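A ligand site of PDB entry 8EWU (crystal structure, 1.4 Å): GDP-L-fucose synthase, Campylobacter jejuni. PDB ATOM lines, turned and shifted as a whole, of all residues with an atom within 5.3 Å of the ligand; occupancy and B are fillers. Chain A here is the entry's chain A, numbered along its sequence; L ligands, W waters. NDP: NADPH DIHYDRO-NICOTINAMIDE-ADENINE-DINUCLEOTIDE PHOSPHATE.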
ATOM      1  N   GLY A  32      -9.860   6.826   9.846  1.00  0.00           N
ATOM      2  CA  GLY A  32      -8.813   7.594   9.148  1.00  0.00           C
ATOM      3  C   GLY A  32      -8.141   6.762   8.063  1.00  0.00           C
ATOM      4  O   GLY A  32      -6.919   6.872   7.885  1.00  0.00           O
ATOM      5  N   HIS A  33      -8.928   5.984   7.306  1.00  0.00           N
ATOM      6  CA  HIS A  33      -8.408   5.011   6.299  1.00  0.00           C
ATOM      7  C   HIS A  33      -7.806   5.743   5.104  1.00  0.00           C
ATOM      8  O   HIS A  33      -7.087   5.049   4.331  1.00  0.00           O
ATOM      9  CB  HIS A  33      -9.493   4.009   5.843  1.00  0.00           C
ATOM     10  CG  HIS A  33     -10.460   4.576   4.874  1.00  0.00           C
ATOM     11  ND1 HIS A  33     -11.530   5.358   5.281  1.00  0.00           N
ATOM     12  CD2 HIS A  33     -10.500   4.550   3.510  1.00  0.00           C
ATOM     13  CE1 HIS A  33     -12.204   5.781   4.216  1.00  0.00           C
ATOM     14  NE2 HIS A  33     -11.580   5.311   3.103  1.00  0.00           N
ATOM     15  N   THR A  34      -8.112   7.017   4.868  1.00  0.00           N
ATOM     16  CA  THR A  34      -7.546   7.773   3.728  1.00  0.00           C
ATOM     17  C   THR A  34      -6.143   8.301   4.070  1.00  0.00           C
ATOM     18  O   THR A  34      -5.464   8.801   3.178  1.00  0.00           O
ATOM     19  CB  THR A  34      -8.482   8.861   3.190  1.00  0.00           C
ATOM     20  OG1 THR A  34      -8.594   9.958   4.102  1.00  0.00           O
ATOM     21  CG2 THR A  34      -9.821   8.293   2.790  1.00  0.00           C
ATOM     22  N   GLY A  35      -5.750   8.260   5.342  1.00  0.00           N
ATOM     23  CA  GLY A  35      -4.477   8.879   5.766  1.00  0.00           C
ATOM     24  C   GLY A  35      -3.259   8.015   5.473  1.00  0.00           C
ATOM     25  O   GLY A  35      -3.382   6.886   4.961  1.00  0.00           O
ATOM     26  N   LEU A  36      -2.111   8.526   5.862  1.00  0.00           N
ATOM     27  CA  LEU A  36      -0.818   7.835   5.650  1.00  0.00           C
ATOM     28  C   LEU A  36      -0.883   6.431   6.241  1.00  0.00           C
ATOM     29  O   LEU A  36      -0.767   5.434   5.503  1.00  0.00           O
ATOM     30  CB  LEU A  36       0.270   8.675   6.324  1.00  0.00           C
ATOM     31  CG  LEU A  36       1.650   8.041   6.396  1.00  0.00           C
ATOM     32  CD1 LEU A  36       2.196   7.778   4.997  1.00  0.00           C
ATOM     33  CD2 LEU A  36       2.570   8.916   7.188  1.00  0.00           C
ATOM     34  N   VAL A  37      -1.114   6.315   7.552  1.00  0.00           N
ATOM     35  CA  VAL A  37      -1.115   5.019   8.246  1.00  0.00           C
ATOM     36  C   VAL A  37      -2.386   4.230   7.924  1.00  0.00           C
ATOM     37  O   VAL A  37      -2.269   3.017   7.633  1.00  0.00           O
ATOM     38  CB  VAL A  37      -0.948   5.210   9.754  1.00  0.00           C
ATOM     39  CG1 VAL A  37      -0.976   3.878  10.454  1.00  0.00           C
ATOM     40  CG2 VAL A  37       0.320   5.980  10.082  1.00  0.00           C
ATOM     41  N   GLY A  38      -3.540   4.857   8.012  1.00  0.00           N
ATOM     42  CA  GLY A  38      -4.793   4.126   7.777  1.00  0.00           C
ATOM     43  C   GLY A  38      -4.825   3.514   6.387  1.00  0.00           C
ATOM     44  O   GLY A  38      -5.309   2.389   6.286  1.00  0.00           O
ATOM     45  N   THR A  57     -15.101   7.694   4.736  1.00  0.00           N
ATOM     46  CA  THR A  57     -14.422   8.970   4.520  1.00  0.00           C
ATOM     47  C   THR A  57     -14.863   9.953   5.601  1.00  0.00           C
ATOM     48  O   THR A  57     -15.932   9.771   6.189  1.00  0.00           O
ATOM     49  CB  THR A  57     -14.704   9.479   3.107  1.00  0.00           C
ATOM     50  OG1 THR A  57     -16.076   9.832   3.029  1.00  0.00           O
ATOM     51  CG2 THR A  57     -14.378   8.428   2.053  1.00  0.00           C
ATOM     52  N   HIS A  58     -14.086  11.015   5.786  1.00  0.00           N
ATOM     53  CA  HIS A  58     -14.447  12.159   6.650  1.00  0.00           C
ATOM     54  C   HIS A  58     -15.810  12.702   6.216  1.00  0.00           C
ATOM     55  O   HIS A  58     -16.645  12.991   7.091  1.00  0.00           O
ATOM     56  CB  HIS A  58     -13.265  13.115   6.561  1.00  0.00           C
ATOM     57  CG  HIS A  58     -13.344  14.360   7.358  1.00  0.00           C
ATOM     58  ND1 HIS A  58     -12.224  15.187   7.492  1.00  0.00           N
ATOM     59  CD2 HIS A  58     -14.367  14.991   7.979  1.00  0.00           C
ATOM     60  CE1 HIS A  58     -12.574  16.242   8.187  1.00  0.00           C
ATOM     61  NE2 HIS A  58     -13.881  16.163   8.484  1.00  0.00           N
ATOM     62  N   LEU A  61     -18.450  10.136   7.507  1.00  0.00           N
ATOM     63  CA  LEU A  61     -18.543  10.082   8.980  1.00  0.00           C
ATOM     64  C   LEU A  61     -17.556  11.071   9.605  1.00  0.00           C
ATOM     65  O   LEU A  61     -16.326  10.822   9.571  1.00  0.00           O
ATOM     66  CB  LEU A  61     -18.229   8.666   9.437  1.00  0.00           C
ATOM     67  CG  LEU A  61     -18.150   8.468  10.950  1.00  0.00           C
ATOM     68  CD1 LEU A  61     -19.442   8.869  11.641  1.00  0.00           C
ATOM     69  CD2 LEU A  61     -17.808   7.020  11.259  1.00  0.00           C
ATOM     70  N   ASP A  62     -18.094  12.165  10.132  1.00  0.00           N
ATOM     71  CA  ASP A  62     -17.279  13.194  10.788  1.00  0.00           C
ATOM     72  C   ASP A  62     -17.062  12.748  12.231  1.00  0.00           C
ATOM     73  O   ASP A  62     -18.013  12.810  13.040  1.00  0.00           O
ATOM     74  CB  ASP A  62     -17.969  14.533  10.652  1.00  0.00           C
ATOM     75  CG  ASP A  62     -17.163  15.660  11.249  1.00  0.00           C
ATOM     76  OD1 ASP A  62     -16.116  15.410  11.861  1.00  0.00           O
ATOM     77  OD2 ASP A  62     -17.593  16.817  11.047  1.00  0.00           O
ATOM     78  N   LEU A  63     -15.830  12.316  12.549  1.00  0.00           N
ATOM     79  CA  LEU A  63     -15.519  11.774  13.879  1.00  0.00           C
ATOM     80  C   LEU A  63     -15.448  12.890  14.911  1.00  0.00           C
ATOM     81  O   LEU A  63     -15.328  12.526  16.066  1.00  0.00           O
ATOM     82  CB  LEU A  63     -14.218  10.971  13.848  1.00  0.00           C
ATOM     83  CG  LEU A  63     -14.280   9.745  12.941  1.00  0.00           C
ATOM     84  CD1 LEU A  63     -12.906   9.133  12.783  1.00  0.00           C
ATOM     85  CD2 LEU A  63     -15.239   8.701  13.492  1.00  0.00           C
ATOM     86  N   THR A  64     -15.658  14.146  14.539  1.00  0.00           N
ATOM     87  CA  THR A  64     -15.821  15.277  15.528  1.00  0.00           C
ATOM     88  C   THR A  64     -17.288  15.478  15.913  1.00  0.00           C
ATOM     89  O   THR A  64     -17.566  16.373  16.743  1.00  0.00           O
ATOM     90  CB  THR A  64     -15.252  16.611  15.045  1.00  0.00           C
ATOM     91  OG1 THR A  64     -15.963  17.085  13.889  1.00  0.00           O
ATOM     92  CG2 THR A  64     -13.770  16.484  14.764  1.00  0.00           C
ATOM     93  N   PHE A  83      -7.431   3.051  15.222  1.00  0.00           N
ATOM     94  CA  PHE A  83      -7.734   4.492  15.301  1.00  0.00           C
ATOM     95  C   PHE A  83      -6.620   5.274  14.615  1.00  0.00           C
ATOM     96  O   PHE A  83      -5.639   5.570  15.269  1.00  0.00           O
ATOM     97  CB  PHE A  83      -7.903   4.945  16.755  1.00  0.00           C
ATOM     98  CG  PHE A  83      -8.255   6.398  16.779  1.00  0.00           C
ATOM     99  CD1 PHE A  83      -9.467   6.832  16.284  1.00  0.00           C
ATOM    100  CD2 PHE A  83      -7.374   7.327  17.297  1.00  0.00           C
ATOM    101  CE1 PHE A  83      -9.796   8.185  16.278  1.00  0.00           C
ATOM    102  CE2 PHE A  83      -7.686   8.673  17.278  1.00  0.00           C
ATOM    103  CZ  PHE A  83      -8.894   9.106  16.750  1.00  0.00           C
ATOM    104  N   CYS A  84      -6.804   5.634  13.349  1.00  0.00           N
ATOM    105  CA  CYS A  84      -5.809   6.304  12.489  1.00  0.00           C
ATOM    106  C   CYS A  84      -6.303   7.664  12.030  1.00  0.00           C
ATOM    107  O   CYS A  84      -5.660   8.227  11.151  1.00  0.00           O
ATOM    108  CB  CYS A  84      -5.437   5.441  11.285  1.00  0.00           C
ATOM    109  SG  CYS A  84      -5.079   3.720  11.679  1.00  0.00           S
ATOM    110  N   ALA A  85      -7.384   8.208  12.616  1.00  0.00           N
ATOM    111  CA  ALA A  85      -7.906   9.548  12.309  1.00  0.00           C
ATOM    112  C   ALA A  85      -7.180  10.573  13.170  1.00  0.00           C
ATOM    113  O   ALA A  85      -6.976  10.329  14.345  1.00  0.00           O
ATOM    114  CB  ALA A  85      -9.407   9.641  12.477  1.00  0.00           C
ATOM    115  N   ALA A  86      -6.906  11.735  12.597  1.00  0.00           N
ATOM    116  CA  ALA A  86      -6.173  12.812  13.260  1.00  0.00           C
ATOM    117  C   ALA A  86      -6.213  14.033  12.384  1.00  0.00           C
ATOM    118  O   ALA A  86      -6.360  13.872  11.172  1.00  0.00           O
ATOM    119  CB  ALA A  86      -4.753  12.405  13.491  1.00  0.00           C
ATOM    120  N   LYS A  87      -6.055  15.173  13.013  1.00  0.00           N
ATOM    121  CA  LYS A  87      -5.768  16.423  12.293  1.00  0.00           C
ATOM    122  C   LYS A  87      -4.423  16.870  12.812  1.00  0.00           C
ATOM    123  O   LYS A  87      -4.372  17.319  13.943  1.00  0.00           O
ATOM    124  CB  LYS A  87      -6.816  17.509  12.501  1.00  0.00           C
ATOM    125  CG  LYS A  87      -6.519  18.808  11.775  1.00  0.00           C
ATOM    126  CD  LYS A  87      -6.411  18.677  10.266  1.00  0.00           C
ATOM    127  CE  LYS A  87      -5.681  19.858   9.658  1.00  0.00           C
ATOM    128  NZ  LYS A  87      -5.774  19.877   8.178  1.00  0.00           N
ATOM    129  N   MET A  88      -3.420  16.795  11.961  1.00  0.00           N
ATOM    130  CA  MET A  88      -2.035  17.168  12.341  1.00  0.00           C
ATOM    131  C   MET A  88      -1.396  18.044  11.277  1.00  0.00           C
ATOM    132  O   MET A  88      -1.979  18.277  10.264  1.00  0.00           O
ATOM    133  CB  MET A  88      -1.122  15.951  12.408  1.00  0.00           C
ATOM    134  CG  MET A  88      -0.865  15.396  11.047  1.00  0.00           C
ATOM    135  SD  MET A  88      -1.628  13.886  11.319  1.00  0.00           S
ATOM    136  CE  MET A  88      -0.722  13.535  12.819  1.00  0.00           C
ATOM    137  N   MET A 108     -12.210  13.496  18.591  1.00  0.00           N
ATOM    138  CA  MET A 108     -12.219  12.294  17.718  1.00  0.00           C
ATOM    139  C   MET A 108     -11.827  11.066  18.529  1.00  0.00           C
ATOM    140  O   MET A 108     -12.548  10.086  18.488  1.00  0.00           O
ATOM    141  CB  MET A 108     -11.307  12.384  16.511  1.00  0.00           C
ATOM    142  CG  MET A 108     -11.835  13.383  15.522  1.00  0.00           C
ATOM    143  SD  MET A 108     -10.943  13.323  13.945  1.00  0.00           S
ATOM    144  CE  MET A 108      -9.569  14.419  14.217  1.00  0.00           C
ATOM    145  N   LEU A 127      -3.137   4.971  18.088  1.00  0.00           N
ATOM    146  CA  LEU A 127      -1.841   5.490  17.636  1.00  0.00           C
ATOM    147  C   LEU A 127      -1.536   6.764  18.392  1.00  0.00           C
ATOM    148  O   LEU A 127      -2.383   7.668  18.441  1.00  0.00           O
ATOM    149  CB  LEU A 127      -1.869   5.760  16.142  1.00  0.00           C
ATOM    150  CG  LEU A 127      -1.655   4.500  15.304  1.00  0.00           C
ATOM    151  CD1 LEU A 127      -2.060   4.765  13.864  1.00  0.00           C
ATOM    152  CD2 LEU A 127      -0.197   4.076  15.371  1.00  0.00           C
ATOM    153  N   SER A 128      -0.376   6.803  19.032  1.00  0.00           N
ATOM    154  CA  SER A 128       0.087   7.950  19.838  1.00  0.00           C
ATOM    155  C   SER A 128       1.298   8.544  19.118  1.00  0.00           C
ATOM    156  O   SER A 128       1.404   8.374  17.877  1.00  0.00           O
ATOM    157  CB  SER A 128       0.307   7.493  21.252  1.00  0.00           C
ATOM    158  OG  SER A 128       0.691   8.545  22.084  1.00  0.00           O
ATOM    159  N   SER A 129       2.147   9.273  19.819  1.00  0.00           N
ATOM    160  CA  SER A 129       3.215  10.052  19.167  1.00  0.00           C
ATOM    161  C   SER A 129       4.332  10.293  20.177  1.00  0.00           C
ATOM    162  O   SER A 129       4.024  10.344  21.374  1.00  0.00           O
ATOM    163  CB  SER A 129       2.661  11.332  18.596  1.00  0.00           C
ATOM    164  OG  SER A 129       3.702  12.278  18.438  1.00  0.00           O
ATOM    165  N   TYR A 158      -0.820  18.863  20.636  1.00  0.00           N
ATOM    166  CA  TYR A 158      -0.964  17.473  20.161  1.00  0.00           C
ATOM    167  C   TYR A 158      -0.463  16.545  21.255  1.00  0.00           C
ATOM    168  O   TYR A 158      -1.112  15.485  21.529  1.00  0.00           O
ATOM    169  CB  TYR A 158      -0.225  17.301  18.848  1.00  0.00           C
ATOM    170  CG  TYR A 158      -0.735  16.116  18.064  1.00  0.00           C
ATOM    171  CD1 TYR A 158      -2.027  16.098  17.580  1.00  0.00           C
ATOM    172  CD2 TYR A 158       0.051  15.016  17.808  1.00  0.00           C
ATOM    173  CE1 TYR A 158      -2.530  15.028  16.858  1.00  0.00           C
ATOM    174  CE2 TYR A 158      -0.416  13.934  17.069  1.00  0.00           C
ATOM    175  CZ  TYR A 158      -1.727  13.927  16.640  1.00  0.00           C
ATOM    176  OH  TYR A 158      -2.226  12.885  15.909  1.00  0.00           O
ATOM    177  N   LYS A 162      -2.486  13.479  22.995  1.00  0.00           N
ATOM    178  CA  LYS A 162      -1.946  12.094  22.947  1.00  0.00           C
ATOM    179  C   LYS A 162      -1.761  11.542  24.343  1.00  0.00           C
ATOM    180  O   LYS A 162      -2.049  10.336  24.612  1.00  0.00           O
ATOM    181  CB  LYS A 162      -0.668  12.022  22.112  1.00  0.00           C
ATOM    182  CG  LYS A 162      -0.912  12.247  20.632  1.00  0.00           C
ATOM    183  CD  LYS A 162      -1.991  11.357  20.066  1.00  0.00           C
ATOM    184  CE  LYS A 162      -1.880  11.128  18.585  1.00  0.00           C
ATOM    185  NZ  LYS A 162      -2.993  10.362  18.024  1.00  0.00           N
ATOM    186  N   PRO A 185       4.674   5.464  17.561  1.00  0.00           N
ATOM    187  CA  PRO A 185       5.685   5.450  16.509  1.00  0.00           C
ATOM    188  C   PRO A 185       6.542   6.720  16.592  1.00  0.00           C
ATOM    189  O   PRO A 185       6.072   7.789  17.013  1.00  0.00           O
ATOM    190  CB  PRO A 185       4.868   5.393  15.210  1.00  0.00           C
ATOM    191  CG  PRO A 185       3.458   5.105  15.657  1.00  0.00           C
ATOM    192  CD  PRO A 185       3.318   5.707  17.028  1.00  0.00           C
ATOM    193  N   THR A 186       7.765   6.587  16.099  1.00  0.00           N
ATOM    194  CA  THR A 186       8.608   7.739  15.685  1.00  0.00           C
ATOM    195  C   THR A 186       7.967   8.427  14.471  1.00  0.00           C
ATOM    196  O   THR A 186       6.902   7.945  13.989  1.00  0.00           O
ATOM    197  CB  THR A 186      10.018   7.275  15.315  1.00  0.00           C
ATOM    198  OG1 THR A 186       9.945   6.510  14.119  1.00  0.00           O
ATOM    199  CG2 THR A 186      10.621   6.397  16.390  1.00  0.00           C
ATOM    200  N   SER A 187       8.590   9.496  13.987  1.00  0.00           N
ATOM    201  CA  SER A 187       8.207  10.132  12.713  1.00  0.00           C
ATOM    202  C   SER A 187       8.114   9.047  11.635  1.00  0.00           C
ATOM    203  O   SER A 187       9.019   8.188  11.558  1.00  0.00           O
ATOM    204  CB  SER A 187       9.168  11.195  12.316  1.00  0.00           C
ATOM    205  OG  SER A 187       9.097  12.302  13.215  1.00  0.00           O
ATOM    206  N   ILE A 188       7.030   9.096  10.844  1.00  0.00           N
ATOM    207  CA  ILE A 188       6.706   8.128   9.779  1.00  0.00           C
ATOM    208  C   ILE A 188       6.944   8.791   8.449  1.00  0.00           C
ATOM    209  O   ILE A 188       6.747  10.004   8.310  1.00  0.00           O
ATOM    210  CB  ILE A 188       5.267   7.604   9.916  1.00  0.00           C
ATOM    211  CG1 ILE A 188       4.947   7.102  11.339  1.00  0.00           C
ATOM    212  CG2 ILE A 188       5.007   6.544   8.862  1.00  0.00           C
ATOM    213  CD1 ILE A 188       3.459   6.657  11.562  1.00  0.00           C
ATOM    214  N   GLY A 192       1.482   8.216   0.491  1.00  0.00           N
ATOM    215  CA  GLY A 192       0.174   8.520   1.106  1.00  0.00           C
ATOM    216  C   GLY A 192       0.271   9.627   2.123  1.00  0.00           C
ATOM    217  O   GLY A 192      -0.781   9.995   2.742  1.00  0.00           O
ATOM    218  N   ASP A 193       1.466  10.161   2.345  1.00  0.00           N
ATOM    219  CA  ASP A 193       1.650  11.248   3.346  1.00  0.00           C
ATOM    220  C   ASP A 193       1.021  12.561   2.837  1.00  0.00           C
ATOM    221  O   ASP A 193       0.660  12.692   1.627  1.00  0.00           O
ATOM    222  CB  ASP A 193       3.142  11.412   3.662  1.00  0.00           C
ATOM    223  CG  ASP A 193       3.475  11.855   5.079  1.00  0.00           C
ATOM    224  OD1 ASP A 193       4.622  11.601   5.506  1.00  0.00           O
ATOM    225  OD2 ASP A 193       2.577  12.463   5.729  1.00  0.00           O
ATOM    226  N   ASN A 194       0.973  13.553   3.721  1.00  0.00           N
ATOM    227  CA  ASN A 194       0.721  14.964   3.379  1.00  0.00           C
ATOM    228  C   ASN A 194       2.043  15.581   2.945  1.00  0.00           C
ATOM    229  O   ASN A 194       2.907  15.699   3.807  1.00  0.00           O
ATOM    230  CB  ASN A 194       0.144  15.696   4.597  1.00  0.00           C
ATOM    231  CG  ASN A 194       0.090  17.181   4.388  1.00  0.00           C
ATOM    232  OD1 ASN A 194      -0.033  17.667   3.241  1.00  0.00           O
ATOM    233  ND2 ASN A 194       0.209  17.907   5.487  1.00  0.00           N
ATOM    234  N   HIS A 201       4.861  17.557   7.792  1.00  0.00           N
ATOM    235  CA  HIS A 201       5.941  17.113   8.708  1.00  0.00           C
ATOM    236  C   HIS A 201       7.299  17.126   7.979  1.00  0.00           C
ATOM    237  O   HIS A 201       7.371  17.268   6.732  1.00  0.00           O
ATOM    238  CB  HIS A 201       5.595  15.741   9.318  1.00  0.00           C
ATOM    239  CG  HIS A 201       4.694  15.898  10.504  1.00  0.00           C
ATOM    240  ND1 HIS A 201       5.175  16.355  11.751  1.00  0.00           N
ATOM    241  CD2 HIS A 201       3.351  15.744  10.650  1.00  0.00           C
ATOM    242  CE1 HIS A 201       4.149  16.416  12.611  1.00  0.00           C
ATOM    243  NE2 HIS A 201       3.021  16.033  11.945  1.00  0.00           N
ATOM    244  N   ARG A 372      -1.293  14.258  -1.896  1.00  0.00           N
ATOM    245  CA  ARG A 372      -1.723  15.288  -0.928  1.00  0.00           C
ATOM    246  C   ARG A 372      -0.709  16.441  -0.925  1.00  0.00           C
ATOM    247  O   ARG A 372       0.413  16.206  -0.486  1.00  0.00           O
ATOM    248  CB  ARG A 372      -1.834  14.641   0.452  1.00  0.00           C
ATOM    249  CG  ARG A 372      -2.876  13.536   0.517  1.00  0.00           C
ATOM    250  CD  ARG A 372      -2.754  12.691   1.767  1.00  0.00           C
ATOM    251  NE  ARG A 372      -3.100  13.458   2.950  1.00  0.00           N
ATOM    252  CZ  ARG A 372      -2.880  13.086   4.200  1.00  0.00           C
ATOM    253  NH1 ARG A 372      -2.241  11.969   4.468  1.00  0.00           N
ATOM    254  NH2 ARG A 372      -3.262  13.900   5.186  1.00  0.00           N
HETATM  255  PA  NDP L   1      -3.013  11.623   8.207  1.00  0.00           P
HETATM  256  O1A NDP L   1      -3.114  13.106   8.256  1.00  0.00           O
HETATM  257  O2A NDP L   1      -2.256  11.099   7.033  1.00  0.00           O
HETATM  258  O5B NDP L   1      -4.457  10.967   8.201  1.00  0.00           O
HETATM  259  C5B NDP L   1      -5.517  11.476   9.048  1.00  0.00           C
HETATM  260  C4B NDP L   1      -6.816  10.762   8.712  1.00  0.00           C
HETATM  261  O4B NDP L   1      -7.837  11.262   9.616  1.00  0.00           O
HETATM  262  C3B NDP L   1      -7.353  11.009   7.310  1.00  0.00           C
HETATM  263  O3B NDP L   1      -8.032   9.841   6.884  1.00  0.00           O
HETATM  264  C2B NDP L   1      -8.286  12.168   7.542  1.00  0.00           C
HETATM  265  O2B NDP L   1      -9.242  12.218   6.430  1.00  0.00           O
HETATM  266  C1B NDP L   1      -8.926  11.646   8.837  1.00  0.00           C
HETATM  267  N9A NDP L   1      -9.715  12.639   9.542  1.00  0.00           N
HETATM  268  C8A NDP L   1      -9.307  13.897   9.914  1.00  0.00           C
HETATM  269  N7A NDP L   1     -10.284  14.612  10.456  1.00  0.00           N
HETATM  270  C5A NDP L   1     -11.370  13.745  10.443  1.00  0.00           C
HETATM  271  C6A NDP L   1     -12.705  13.896  10.873  1.00  0.00           C
HETATM  272  N6A NDP L   1     -13.179  15.022  11.429  1.00  0.00           N
HETATM  273  N1A NDP L   1     -13.527  12.819  10.746  1.00  0.00           N
HETATM  274  C2A NDP L   1     -13.044  11.698  10.176  1.00  0.00           C
HETATM  275  N3A NDP L   1     -11.823  11.469   9.679  1.00  0.00           N
HETATM  276  C4A NDP L   1     -11.029  12.536   9.891  1.00  0.00           C
HETATM  277  O3  NDP L   1      -2.355  11.083   9.556  1.00  0.00           O
HETATM  278  PN  NDP L   1      -1.255   9.961   9.784  1.00  0.00           P
HETATM  279  O1N NDP L   1       0.116  10.589   9.602  1.00  0.00           O
HETATM  280  O2N NDP L   1      -1.694   8.727   9.049  1.00  0.00           O
HETATM  281  O5D NDP L   1      -1.443   9.724  11.365  1.00  0.00           O
HETATM  282  C5D NDP L   1      -2.269   8.643  11.840  1.00  0.00           C
HETATM  283  C4D NDP L   1      -1.983   8.516  13.314  1.00  0.00           C
HETATM  284  O4D NDP L   1      -0.614   8.098  13.454  1.00  0.00           O
HETATM  285  C3D NDP L   1      -2.145   9.806  14.172  1.00  0.00           C
HETATM  286  O3D NDP L   1      -2.674   9.534  15.474  1.00  0.00           O
HETATM  287  C2D NDP L   1      -0.719  10.232  14.313  1.00  0.00           C
HETATM  288  O2D NDP L   1      -0.465  11.079  15.429  1.00  0.00           O
HETATM  289  C1D NDP L   1       0.020   8.937  14.381  1.00  0.00           C
HETATM  290  N1N NDP L   1       1.439   9.051  14.025  1.00  0.00           N
HETATM  291  C2N NDP L   1       1.849   9.616  12.839  1.00  0.00           C
HETATM  292  C3N NDP L   1       3.176  10.007  12.662  1.00  0.00           C
HETATM  293  C7N NDP L   1       3.667  10.541  11.390  1.00  0.00           C
HETATM  294  O7N NDP L   1       4.844  10.953  11.330  1.00  0.00           O
HETATM  295  N7N NDP L   1       2.835  10.608  10.360  1.00  0.00           N
HETATM  296  C4N NDP L   1       4.173   9.829  13.758  1.00  0.00           C
HETATM  297  C5N NDP L   1       3.660   9.018  14.858  1.00  0.00           C
HETATM  298  C6N NDP L   1       2.387   8.793  15.017  1.00  0.00           C
HETATM  299  P2B NDP L   1      -9.312  13.638   5.655  1.00  0.00           P
HETATM  300  O1X NDP L   1      -7.954  13.974   5.197  1.00  0.00           O
HETATM  301  O2X NDP L   1      -9.816  14.675   6.607  1.00  0.00           O
HETATM  302  O3X NDP L   1     -10.337  13.314   4.571  1.00  0.00           O
HETATM  303  O   HOH W   1      -5.773  15.076   5.767  1.00  0.00           O
HETATM  304  O   HOH W   2      -4.043   7.520   8.658  1.00  0.00           O
HETATM  305  O   HOH W   3     -12.140  14.790   3.540  1.00  0.00           O
HETATM  306  O   HOH W   4     -14.607   8.916   8.766  1.00  0.00           O
HETATM  307  O   HOH W   5      -5.054   8.434  15.070  1.00  0.00           O
HETATM  308  O   HOH W   6      -6.881  11.841   3.827  1.00  0.00           O
HETATM  309  O   HOH W   7       4.694  11.914   8.213  1.00  0.00           O
HETATM  310  O   HOH W   8      -4.401  15.347   9.294  1.00  0.00           O
HETATM  311  O   HOH W   9       2.074  12.432  15.260  1.00  0.00           O
HETATM  312  O   HOH W  10      -0.636  14.435   7.788  1.00  0.00           O
HETATM  313  O   HOH W  11     -11.747   8.847   8.647  1.00  0.00           O
HETATM  314  O   HOH W  12     -11.518  10.918   4.464  1.00  0.00           O
HETATM  315  O   HOH W  13     -10.765   8.230   6.041  1.00  0.00           O
HETATM  316  O   HOH W  14       1.122  12.456   8.011  1.00  0.00           O
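Water W1 bridges O1X of the ligand and NH2 of Arg 372.
Water W5 lies within hydrogen-bond range of an oxygen (O3D) of the ligand (2.7 Å), the backbone carbonyl oxygen (O) of Ala 85 (2.8 Å) and the backbone carbonyl oxygen (O) of Phe 83 (2.9 Å).
Water W12 lies within hydrogen-bond range of O3X of the ligand (2.7 Å), N of His 58 (2.9 Å) and OG1 of Thr 34 (3.1 Å).
Water W11 lies within hydrogen-bond range of N3A of the ligand (2.8 Å) and N of Gly 32 (3.0 Å).
Water W10 lies within hydrogen-bond range of O1A of the ligand (2.9 Å) and SD of Met 88 (3.7 Å).
Water W13 lies within hydrogen-bond range of a ring nitrogen (ND1) of His 33 (3.1 Å), the backbone NH of Thr 34 (3.1 Å) and an oxygen (O3B) of the ligand (3.3 Å).
OH of Tyr 158 sits close to NZ of Lys 162, at 3.4 Å.
The side-chain amino group (NZ) of Lys 162 sits at hydrogen-bond distance from the backbone carbonyl oxygen (O) of Leu 127 (2.8 Å).
The guanidinium group (NH1) of Arg 372 is in hydrogen-bond range of the backbone carbonyl oxygen (O) of Gly 192.
OD1 of Asp 62 lies within hydrogen-bond range of OG1 of Thr 64 (2.6 Å).
The side-chain hydroxyl of Tyr 158 is in hydrogen-bond range of an oxygen (O2D) of the ligand (2.6 Å).
O2X of the ligand lies within hydrogen-bond range of ND1 of His 58, at 2.6 Å.
NZ of Lys 162 sits at hydrogen-bond distance from O3D of the ligand, at 2.7 Å.
The guanidinium group of Arg 372 is in salt-bridge range of an oxygen (O2A) of the ligand, at 2.7 Å.
N of Leu 36 lies within hydrogen-bond range of O2A of the ligand (2.8 Å).
The backbone NH (N) of Thr 34 lies within hydrogen-bond range of an oxygen (O3B) of the ligand (3.5 Å).
OG1 of Thr 34 lies within hydrogen-bond range of O3B of the ligand, at 2.8 Å.
O2N of the ligand lies within hydrogen-bond range of N of Val 37 (2.9 Å).
An oxygen (O7N) of the ligand lies within hydrogen-bond range of the backbone NH (N) of Ile 188.
The backbone NH (N) of Leu 63 sits at hydrogen-bond distance from a nitrogen (N1A) of the ligand, at 3.0 Å.
The side-chain carboxylate (OD1) of Asp 62 lies within hydrogen-bond range of a nitrogen (N6A) of the ligand, 3.0 Å away.
The backbone NH (N) of Ala 86 lies within hydrogen-bond range of an oxygen (O4B) of the ligand (3.2 Å).
O3B of the ligand is in hydrogen-bond range of N of Gly 35, 3.2 Å away.
The backbone carbonyl oxygen (O) of Gly 32 sits close to an oxygen (O3B) of the ligand.
SD of Met 108 lies close to N6A of the ligand (3.8 Å).
O3 of the ligand lies close to SD of Met 88 (3.4 Å).
His 33 touches the ligand.
Leu 61 touches the ligand.
Thr 64 touches the ligand.
O of Cys 84 touches C5D of the ligand, at 3.5 Å.
Ala 85 touches the ligand.
Leu 127 touches the ligand.
Ser 128 touches the ligand (O to C6N, 3.1 Å).
Pro 185 touches the ligand.
Thr 186 touches the ligand (O to C4N, 3.3 Å).
Ser 187 touches the ligand.
Hydrophobic or aromatic side chains that line the ligand: Leu 36, Val 37, His 58, Leu 63, Ala 85, Ala 86, Met 88, Met 108, Leu 127, Tyr 158, Pro 185 and Ile 188.
25 residues have an atom within 4 Å of the ligand: Gly 32, His 33, Thr 34, Gly 35, Leu 36, Val 37, His 58, Leu 61, Asp 62, Leu 63, Thr 64, Cys 84, Ala 85, Ala 86, Met 88, Met 108, Leu 127, Ser 128, Tyr 158, Lys 162, Pro 185, Thr 186, Ser 187, Ile 188 and Arg 372.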
